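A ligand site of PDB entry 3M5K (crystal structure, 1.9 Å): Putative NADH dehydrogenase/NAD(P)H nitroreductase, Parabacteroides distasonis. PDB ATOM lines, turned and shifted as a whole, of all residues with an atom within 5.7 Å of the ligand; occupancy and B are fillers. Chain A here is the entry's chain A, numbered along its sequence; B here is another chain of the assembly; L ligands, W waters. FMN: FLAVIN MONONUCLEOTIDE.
NE of Arg 19 lies within hydrogen-bond range of O2 of the ligand, 2.8 Å away.
A nitrogen (N5) of the ligand sits at hydrogen-bond distance from the backbone NH (N) of Ala 120 (3.2 Å).
The backbone NH (N) of Ser 43 of chain B is in hydrogen-bond range of an oxygen (O3') of the ligand (3.1 Å).
The side-chain amino group of Lys 159 is in salt-bridge range of an oxygen (O3P) of the ligand.
NH1 of Arg 15 lies within salt-bridge range of O2P of the ligand, at 2.8 Å.
An oxygen (O2P) of the ligand sits at hydrogen-bond distance from the side-chain hydroxyl (OG) of Ser 17.
The side-chain amino group of Lys 161 lies within salt-bridge range of an oxygen (O1P) of the ligand (2.7 Å).
An oxygen (O3P) of the ligand lies within hydrogen-bond range of the backbone NH of Ser 17.
The guanidinium group (NH1) of Arg 127 lies within hydrogen-bond range of an oxygen (O4) of the ligand (3.3 Å).
The backbone carbonyl oxygen (O) of Phe 70 lies within hydrogen-bond range of a nitrogen (N3) of the ligand, 2.9 Å away.
The backbone carbonyl oxygen (O) of Ala 120 is in hydrogen-bond range of the guanidinium group (NH1) of Arg 127 (3.2 Å).
O of Ala 41 of chain B sits at hydrogen-bond distance from NZ of Lys 161, at 2.8 Å.
The side-chain amino group (NZ) of Lys 161 sits at hydrogen-bond distance from the backbone carbonyl oxygen (O) of Ala 40 of chain B (3.4 Å).
The side-chain carboxylate (OD2) of Asp 97 of chain B lies within hydrogen-bond range of the side-chain hydroxyl (OG) of Ser 43 of chain B (2.7 Å).
The guanidinium group (NH2) of Arg 15 sits at hydrogen-bond distance from the backbone carbonyl oxygen (O) of Ala 40 of chain B.
OD1 of Asp 97 of chain B is in hydrogen-bond range of N of Ser 44 of chain B, 2.9 Å away.
A nitrogen (N10) of the ligand sits close to the backbone carbonyl oxygen of Trp 118 (2.8 Å).
Residues that only touch the ligand: Pro 42 of chain B (3.2 Å), Lys 16 (3.4 Å), Ser 44 of chain B (3.4 Å), Asp 97 of chain B (3.5 Å), Asp 46 of chain B (3.5 Å), Thr 119 (3.5 Å), Val 117 (3.6 Å) and Met 73 (3.7 Å).
Hydrophobic or aromatic side chains within 4 Å of the ligand: Phe 70, Met 73, Val 117, Trp 118, Ala 120 and Pro 42 of chain B.
18 residues have an atom within 4 Å of the ligand: Arg 15, Lys 16, Ser 17, Arg 19, Phe 70, Met 73, Val 117, Trp 118, Thr 119, Ala 120, Arg 127, Lys 159, Lys 161, Pro 42 of chain B, Ser 43 of chain B, Ser 44 of chain B, Asp 46 of chain B and Asp 97 of chain B.
Water W2 bridges O2 of the ligand (2.7 Å) and O of Phe 70 (3.0 Å).
Water W3 lies within hydrogen-bond range of O4' of the ligand (2.8 Å), NH1 of Arg 19 (3.1 Å) and NZ of Lys 159 (3.2 Å).
Water W1 lies within hydrogen-bond range of the backbone NH of Lys 159, the backbone carbonyl oxygen of Arg 15 and an oxygen (O1P) of the ligand.
Water W4 lies within hydrogen-bond range of NH1 of Arg 127, O4 of the ligand and O of Ala 120.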
ATOM      1  N   ARG A  15     -18.753  12.918  28.139  1.00  0.00           N
ATOM      2  CA  ARG A  15     -18.577  11.867  27.130  1.00  0.00           C
ATOM      3  C   ARG A  15     -19.933  11.509  26.462  1.00  0.00           C
ATOM      4  O   ARG A  15     -20.959  11.376  27.149  1.00  0.00           O
ATOM      5  CB  ARG A  15     -17.930  10.631  27.765  1.00  0.00           C
ATOM      6  CG  ARG A  15     -17.604   9.494  26.770  1.00  0.00           C
ATOM      7  CD  ARG A  15     -17.838   8.061  27.384  1.00  0.00           C
ATOM      8  NE  ARG A  15     -19.165   7.970  27.973  1.00  0.00           N
ATOM      9  CZ  ARG A  15     -20.281   7.743  27.289  1.00  0.00           C
ATOM     10  NH1 ARG A  15     -20.251   7.516  25.988  1.00  0.00           N
ATOM     11  NH2 ARG A  15     -21.452   7.737  27.926  1.00  0.00           N
ATOM     12  N   LYS A  16     -19.942  11.355  25.146  1.00  0.00           N
ATOM     13  CA  LYS A  16     -21.096  10.803  24.438  1.00  0.00           C
ATOM     14  C   LYS A  16     -20.642   9.961  23.264  1.00  0.00           C
ATOM     15  O   LYS A  16     -19.523  10.081  22.828  1.00  0.00           O
ATOM     16  CB  LYS A  16     -22.030  11.924  23.932  1.00  0.00           C
ATOM     17  CG  LYS A  16     -21.464  12.801  22.777  1.00  0.00           C
ATOM     18  CD  LYS A  16     -21.083  14.179  23.309  1.00  0.00           C
ATOM     19  CE  LYS A  16     -19.670  14.334  23.442  1.00  0.00           C
ATOM     20  NZ  LYS A  16     -19.369  15.662  23.968  1.00  0.00           N
ATOM     21  N   SER A  17     -21.533   9.092  22.783  1.00  0.00           N
ATOM     22  CA  SER A  17     -21.265   8.272  21.607  1.00  0.00           C
ATOM     23  C   SER A  17     -21.292   9.200  20.372  1.00  0.00           C
ATOM     24  O   SER A  17     -22.262   9.943  20.190  1.00  0.00           O
ATOM     25  CB  SER A  17     -22.281   7.158  21.492  1.00  0.00           C
ATOM     26  OG  SER A  17     -22.060   6.164  22.480  1.00  0.00           O
ATOM     27  N   ARG A  19     -20.982   9.199  16.277  1.00  0.00           N
ATOM     28  CA  ARG A  19     -21.129   8.289  15.135  1.00  0.00           C
ATOM     29  C   ARG A  19     -20.910   8.948  13.753  1.00  0.00           C
ATOM     30  O   ARG A  19     -21.077   8.280  12.726  1.00  0.00           O
ATOM     31  CB  ARG A  19     -22.502   7.655  15.197  1.00  0.00           C
ATOM     32  CG  ARG A  19     -22.760   6.850  16.512  1.00  0.00           C
ATOM     33  CD  ARG A  19     -24.075   6.083  16.477  1.00  0.00           C
ATOM     34  NE  ARG A  19     -24.294   5.268  17.658  1.00  0.00           N
ATOM     35  CZ  ARG A  19     -24.769   5.734  18.808  1.00  0.00           C
ATOM     36  NH1 ARG A  19     -25.065   7.026  18.963  1.00  0.00           N
ATOM     37  NH2 ARG A  19     -24.920   4.925  19.843  1.00  0.00           N
ATOM     38  N   PHE A  70     -25.331  -2.558  13.484  1.00  0.00           N
ATOM     39  CA  PHE A  70     -25.248  -1.306  14.270  1.00  0.00           C
ATOM     40  C   PHE A  70     -23.912  -0.612  14.253  1.00  0.00           C
ATOM     41  O   PHE A  70     -23.595   0.227  15.112  1.00  0.00           O
ATOM     42  CB  PHE A  70     -25.772  -1.595  15.675  1.00  0.00           C
ATOM     43  CG  PHE A  70     -27.151  -2.146  15.643  1.00  0.00           C
ATOM     44  CD1 PHE A  70     -28.218  -1.328  15.302  1.00  0.00           C
ATOM     45  CD2 PHE A  70     -27.379  -3.503  15.831  1.00  0.00           C
ATOM     46  CE1 PHE A  70     -29.505  -1.830  15.209  1.00  0.00           C
ATOM     47  CE2 PHE A  70     -28.663  -4.018  15.743  1.00  0.00           C
ATOM     48  CZ  PHE A  70     -29.735  -3.170  15.437  1.00  0.00           C
ATOM     49  N   ALA A  71     -23.122  -0.929  13.221  1.00  0.00           N
ATOM     50  CA  ALA A  71     -21.790  -0.359  13.084  1.00  0.00           C
ATOM     51  C   ALA A  71     -21.566   0.108  11.640  1.00  0.00           C
ATOM     52  O   ALA A  71     -20.460   0.045  11.112  1.00  0.00           O
ATOM     53  CB  ALA A  71     -20.710  -1.373  13.548  1.00  0.00           C
ATOM     54  N   MET A  73     -21.350   3.011  10.512  1.00  0.00           N
ATOM     55  CA  MET A  73     -20.454   4.170  10.520  1.00  0.00           C
ATOM     56  C   MET A  73     -18.988   3.838  10.246  1.00  0.00           C
ATOM     57  O   MET A  73     -18.184   4.730   9.933  1.00  0.00           O
ATOM     58  CB  MET A  73     -20.603   4.966  11.834  1.00  0.00           C
ATOM     59  CG  MET A  73     -19.784   4.465  13.033  1.00  0.00           C
ATOM     60  SD  MET A  73     -20.469   2.779  13.682  1.00  0.00           S
ATOM     61  CE  MET A  73     -22.026   3.488  14.619  1.00  0.00           C
ATOM     62  N   VAL A 117     -17.395   5.690  19.573  1.00  0.00           N
ATOM     63  CA  VAL A 117     -18.569   4.954  19.976  1.00  0.00           C
ATOM     64  C   VAL A 117     -18.215   3.498  20.156  1.00  0.00           C
ATOM     65  O   VAL A 117     -17.491   2.907  19.339  1.00  0.00           O
ATOM     66  CB  VAL A 117     -19.759   5.075  18.970  1.00  0.00           C
ATOM     67  CG1 VAL A 117     -19.340   4.587  17.545  1.00  0.00           C
ATOM     68  CG2 VAL A 117     -21.034   4.329  19.526  1.00  0.00           C
ATOM     69  N   TRP A 118     -18.684   2.933  21.257  1.00  0.00           N
ATOM     70  CA  TRP A 118     -18.538   1.503  21.545  1.00  0.00           C
ATOM     71  C   TRP A 118     -19.629   0.756  20.755  1.00  0.00           C
ATOM     72  O   TRP A 118     -20.820   0.958  21.011  1.00  0.00           O
ATOM     73  CB  TRP A 118     -18.718   1.317  23.039  1.00  0.00           C
ATOM     74  CG  TRP A 118     -18.704  -0.085  23.583  1.00  0.00           C
ATOM     75  CD1 TRP A 118     -19.190  -1.251  22.996  1.00  0.00           C
ATOM     76  CD2 TRP A 118     -18.285  -0.450  24.893  1.00  0.00           C
ATOM     77  NE1 TRP A 118     -19.035  -2.297  23.859  1.00  0.00           N
ATOM     78  CE2 TRP A 118     -18.486  -1.836  25.037  1.00  0.00           C
ATOM     79  CE3 TRP A 118     -17.744   0.276  25.979  1.00  0.00           C
ATOM     80  CZ2 TRP A 118     -18.159  -2.526  26.220  1.00  0.00           C
ATOM     81  CZ3 TRP A 118     -17.426  -0.418  27.160  1.00  0.00           C
ATOM     82  CH2 TRP A 118     -17.644  -1.793  27.264  1.00  0.00           C
ATOM     83  N   THR A 119     -19.231  -0.070  19.793  1.00  0.00           N
ATOM     84  CA  THR A 119     -20.184  -0.926  19.062  1.00  0.00           C
ATOM     85  C   THR A 119     -19.918  -2.365  19.452  1.00  0.00           C
ATOM     86  O   THR A 119     -18.780  -2.844  19.400  1.00  0.00           O
ATOM     87  CB  THR A 119     -20.204  -0.717  17.522  1.00  0.00           C
ATOM     88  OG1 THR A 119     -19.053  -1.294  16.891  1.00  0.00           O
ATOM     89  CG2 THR A 119     -20.289   0.820  17.197  1.00  0.00           C
ATOM     90  N   ALA A 120     -20.973  -3.060  19.836  1.00  0.00           N
ATOM     91  CA  ALA A 120     -20.827  -4.390  20.409  1.00  0.00           C
ATOM     92  C   ALA A 120     -20.415  -5.432  19.374  1.00  0.00           C
ATOM     93  O   ALA A 120     -20.859  -5.376  18.233  1.00  0.00           O
ATOM     94  CB  ALA A 120     -22.138  -4.842  21.081  1.00  0.00           C
ATOM     95  N   ARG A 127     -21.846 -11.216  14.926  1.00  0.00           N
ATOM     96  CA  ARG A 127     -20.890 -10.114  14.933  1.00  0.00           C
ATOM     97  C   ARG A 127     -19.488 -10.646  15.191  1.00  0.00           C
ATOM     98  O   ARG A 127     -18.531 -10.198  14.539  1.00  0.00           O
ATOM     99  CB  ARG A 127     -21.279  -9.071  15.959  1.00  0.00           C
ATOM    100  CG  ARG A 127     -22.718  -8.579  15.845  1.00  0.00           C
ATOM    101  CD  ARG A 127     -22.919  -7.282  16.655  1.00  0.00           C
ATOM    102  NE  ARG A 127     -24.326  -7.078  16.986  1.00  0.00           N
ATOM    103  CZ  ARG A 127     -24.826  -6.086  17.730  1.00  0.00           C
ATOM    104  NH1 ARG A 127     -24.035  -5.153  18.244  1.00  0.00           N
ATOM    105  NH2 ARG A 127     -26.138  -6.036  17.967  1.00  0.00           N
ATOM    106  N   LYS A 159     -25.797  12.775  27.323  1.00  0.00           N
ATOM    107  CA  LYS A 159     -27.032  12.444  28.020  1.00  0.00           C
ATOM    108  C   LYS A 159     -26.805  12.643  29.511  1.00  0.00           C
ATOM    109  O   LYS A 159     -25.689  12.387  30.004  1.00  0.00           O
ATOM    110  CB  LYS A 159     -27.461  11.008  27.723  1.00  0.00           C
ATOM    111  CG  LYS A 159     -27.638  10.749  26.230  1.00  0.00           C
ATOM    112  CD  LYS A 159     -27.918   9.315  25.921  1.00  0.00           C
ATOM    113  CE  LYS A 159     -27.985   9.041  24.374  1.00  0.00           C
ATOM    114  NZ  LYS A 159     -26.799   9.601  23.632  1.00  0.00           N
ATOM    115  N   LYS A 161     -27.846  10.988  32.680  1.00  0.00           N
ATOM    116  CA  LYS A 161     -28.426   9.702  33.041  1.00  0.00           C
ATOM    117  C   LYS A 161     -28.660   9.575  34.568  1.00  0.00           C
ATOM    118  O   LYS A 161     -29.063   8.515  35.040  1.00  0.00           O
ATOM    119  CB  LYS A 161     -27.478   8.586  32.587  1.00  0.00           C
ATOM    120  CG  LYS A 161     -27.110   8.567  31.091  1.00  0.00           C
ATOM    121  CD  LYS A 161     -26.588   7.185  30.669  1.00  0.00           C
ATOM    122  CE  LYS A 161     -25.988   7.154  29.248  1.00  0.00           C
ATOM    123  NZ  LYS A 161     -24.631   7.704  29.235  1.00  0.00           N
ATOM    124  N   ALA B  40     -22.987   7.884  34.252  1.00  0.00           N
ATOM    125  CA  ALA B  40     -22.626   8.489  32.987  1.00  0.00           C
ATOM    126  C   ALA B  40     -22.001   7.516  31.952  1.00  0.00           C
ATOM    127  O   ALA B  40     -21.642   7.949  30.852  1.00  0.00           O
ATOM    128  CB  ALA B  40     -21.667   9.686  33.212  1.00  0.00           C
ATOM    129  N   ALA B  41     -21.836   6.256  32.317  1.00  0.00           N
ATOM    130  CA  ALA B  41     -21.261   5.249  31.428  1.00  0.00           C
ATOM    131  C   ALA B  41     -22.105   5.097  30.149  1.00  0.00           C
ATOM    132  O   ALA B  41     -23.319   5.393  30.160  1.00  0.00           O
ATOM    133  CB  ALA B  41     -21.143   3.878  32.156  1.00  0.00           C
ATOM    134  N   PRO B  42     -21.472   4.626  29.072  1.00  0.00           N
ATOM    135  CA  PRO B  42     -22.243   4.192  27.904  1.00  0.00           C
ATOM    136  C   PRO B  42     -23.044   2.933  28.274  1.00  0.00           C
ATOM    137  O   PRO B  42     -22.720   2.259  29.278  1.00  0.00           O
ATOM    138  CB  PRO B  42     -21.142   3.868  26.867  1.00  0.00           C
ATOM    139  CG  PRO B  42     -19.954   3.422  27.718  1.00  0.00           C
ATOM    140  CD  PRO B  42     -20.025   4.350  28.921  1.00  0.00           C
ATOM    141  N   SER B  43     -24.078   2.624  27.505  1.00  0.00           N
ATOM    142  CA  SER B  43     -24.960   1.496  27.819  1.00  0.00           C
ATOM    143  C   SER B  43     -25.508   0.882  26.541  1.00  0.00           C
ATOM    144  O   SER B  43     -26.044   1.599  25.685  1.00  0.00           O
ATOM    145  CB  SER B  43     -26.151   1.980  28.691  1.00  0.00           C
ATOM    146  OG  SER B  43     -27.129   0.973  28.877  1.00  0.00           O
ATOM    147  N   SER B  44     -25.401  -0.437  26.416  1.00  0.00           N
ATOM    148  CA  SER B  44     -25.986  -1.152  25.267  1.00  0.00           C
ATOM    149  C   SER B  44     -27.491  -0.808  25.117  1.00  0.00           C
ATOM    150  O   SER B  44     -28.305  -1.008  26.018  1.00  0.00           O
ATOM    151  CB  SER B  44     -25.768  -2.643  25.380  1.00  0.00           C
ATOM    152  OG  SER B  44     -26.557  -3.333  24.425  1.00  0.00           O
ATOM    153  N   ARG B  45     -27.843  -0.291  23.944  1.00  0.00           N
ATOM    154  CA  ARG B  45     -29.211   0.162  23.631  1.00  0.00           C
ATOM    155  C   ARG B  45     -29.753   1.214  24.608  1.00  0.00           C
ATOM    156  O   ARG B  45     -30.966   1.419  24.699  1.00  0.00           O
ATOM    157  CB  ARG B  45     -30.175  -1.030  23.529  1.00  0.00           C
ATOM    158  CG  ARG B  45     -29.948  -1.885  22.291  1.00  0.00           C
ATOM    159  CD  ARG B  45     -30.329  -3.332  22.529  1.00  0.00           C
ATOM    160  NE  ARG B  45     -31.771  -3.527  22.660  1.00  0.00           N
ATOM    161  CZ  ARG B  45     -32.366  -4.700  22.873  1.00  0.00           C
ATOM    162  NH1 ARG B  45     -31.669  -5.837  22.985  1.00  0.00           N
ATOM    163  NH2 ARG B  45     -33.696  -4.746  22.967  1.00  0.00           N
ATOM    164  N   ASP B  46     -28.846   1.908  25.276  1.00  0.00           N
ATOM    165  CA  ASP B  46     -29.181   2.857  26.329  1.00  0.00           C
ATOM    166  C   ASP B  46     -30.173   2.320  27.355  1.00  0.00           C
ATOM    167  O   ASP B  46     -31.102   3.030  27.785  1.00  0.00           O
ATOM    168  CB  ASP B  46     -29.655   4.197  25.740  1.00  0.00           C
ATOM    169  CG  ASP B  46     -29.414   5.389  26.673  1.00  0.00           C
ATOM    170  OD1 ASP B  46     -28.648   5.242  27.663  1.00  0.00           O
ATOM    171  OD2 ASP B  46     -29.953   6.496  26.393  1.00  0.00           O
ATOM    172  N   ALA B  93     -26.032  -7.860  28.113  1.00  0.00           N
ATOM    173  CA  ALA B  93     -24.924  -6.924  28.243  1.00  0.00           C
ATOM    174  C   ALA B  93     -24.825  -6.200  29.596  1.00  0.00           C
ATOM    175  O   ALA B  93     -23.981  -5.309  29.734  1.00  0.00           O
ATOM    176  CB  ALA B  93     -24.937  -5.898  27.063  1.00  0.00           C
ATOM    177  N   LEU B  96     -21.301  -5.747  31.031  1.00  0.00           N
ATOM    178  CA  LEU B  96     -20.432  -4.870  30.234  1.00  0.00           C
ATOM    179  C   LEU B  96     -20.709  -3.416  30.594  1.00  0.00           C
ATOM    180  O   LEU B  96     -19.796  -2.649  30.955  1.00  0.00           O
ATOM    181  CB  LEU B  96     -20.640  -5.158  28.727  1.00  0.00           C
ATOM    182  CG  LEU B  96     -20.471  -6.610  28.263  1.00  0.00           C
ATOM    183  CD1 LEU B  96     -20.800  -6.732  26.745  1.00  0.00           C
ATOM    184  CD2 LEU B  96     -19.037  -7.142  28.632  1.00  0.00           C
ATOM    185  N   ASP B  97     -21.986  -3.029  30.521  1.00  0.00           N
ATOM    186  CA  ASP B  97     -22.431  -1.703  30.956  1.00  0.00           C
ATOM    187  C   ASP B  97     -21.950  -1.401  32.399  1.00  0.00           C
ATOM    188  O   ASP B  97     -21.396  -0.332  32.674  1.00  0.00           O
ATOM    189  CB  ASP B  97     -23.963  -1.647  31.007  1.00  0.00           C
ATOM    190  CG  ASP B  97     -24.635  -1.572  29.641  1.00  0.00           C
ATOM    191  OD1 ASP B  97     -24.005  -1.775  28.551  1.00  0.00           O
ATOM    192  OD2 ASP B  97     -25.851  -1.292  29.689  1.00  0.00           O
ATOM    193  N   ALA B 100     -18.185  -0.688  32.684  1.00  0.00           N
ATOM    194  CA  ALA B 100     -17.899   0.697  32.260  1.00  0.00           C
ATOM    195  C   ALA B 100     -18.271   1.705  33.359  1.00  0.00           C
ATOM    196  O   ALA B 100     -17.507   2.633  33.639  1.00  0.00           O
ATOM    197  CB  ALA B 100     -18.649   1.018  30.922  1.00  0.00           C
HETATM  198  N1  FMN L   1     -23.795   1.958  19.724  1.00  0.00           N
HETATM  199  C2  FMN L   1     -23.960   1.627  18.386  1.00  0.00           C
HETATM  200  O2  FMN L   1     -24.145   2.492  17.519  1.00  0.00           O
HETATM  201  N3  FMN L   1     -23.885   0.305  17.995  1.00  0.00           N
HETATM  202  C4  FMN L   1     -23.716  -0.736  18.883  1.00  0.00           C
HETATM  203  O4  FMN L   1     -23.665  -1.874  18.440  1.00  0.00           O
HETATM  204  C4A FMN L   1     -23.572  -0.423  20.244  1.00  0.00           C
HETATM  205  N5  FMN L   1     -23.426  -1.435  21.209  1.00  0.00           N
HETATM  206  C5A FMN L   1     -23.084  -1.063  22.498  1.00  0.00           C
HETATM  207  C6  FMN L   1     -22.738  -2.067  23.403  1.00  0.00           C
HETATM  208  C7  FMN L   1     -22.331  -1.783  24.712  1.00  0.00           C
HETATM  209  C7M FMN L   1     -21.966  -2.999  25.568  1.00  0.00           C
HETATM  210  C8  FMN L   1     -22.258  -0.407  25.136  1.00  0.00           C
HETATM  211  C8M FMN L   1     -21.829   0.035  26.528  1.00  0.00           C
HETATM  212  C9  FMN L   1     -22.615   0.586  24.249  1.00  0.00           C
HETATM  213  C9A FMN L   1     -23.041   0.288  22.899  1.00  0.00           C
HETATM  214  N10 FMN L   1     -23.437   1.294  21.971  1.00  0.00           N
HETATM  215  C10 FMN L   1     -23.618   0.941  20.644  1.00  0.00           C
HETATM  216  C1' FMN L   1     -23.514   2.758  22.325  1.00  0.00           C
HETATM  217  C2' FMN L   1     -24.828   3.016  23.079  1.00  0.00           C
HETATM  218  O2' FMN L   1     -25.918   3.131  22.176  1.00  0.00           O
HETATM  219  C3' FMN L   1     -24.714   4.296  23.934  1.00  0.00           C
HETATM  220  O3' FMN L   1     -23.690   4.187  24.901  1.00  0.00           O
HETATM  221  C4' FMN L   1     -26.048   4.697  24.575  1.00  0.00           C
HETATM  222  O4' FMN L   1     -27.026   5.031  23.578  1.00  0.00           O
HETATM  223  C5' FMN L   1     -25.824   5.860  25.538  1.00  0.00           C
HETATM  224  O5' FMN L   1     -25.376   7.015  24.848  1.00  0.00           O
HETATM  225  P   FMN L   1     -23.987   7.767  25.178  1.00  0.00           P
HETATM  226  O1P FMN L   1     -24.071   8.220  26.630  1.00  0.00           O
HETATM  227  O2P FMN L   1     -22.794   6.847  24.913  1.00  0.00           O
HETATM  228  O3P FMN L   1     -23.901   8.920  24.224  1.00  0.00           O
HETATM  229  O   HOH W   1     -23.740  11.007  27.012  1.00  0.00           O
HETATM  230  O   HOH W   2     -25.512   2.573  15.183  1.00  0.00           O
HETATM  231  O   HOH W   3     -26.602   7.040  21.698  1.00  0.00           O
HETATM  232  O   HOH W   4     -22.672  -3.563  15.877  1.00  0.00           O
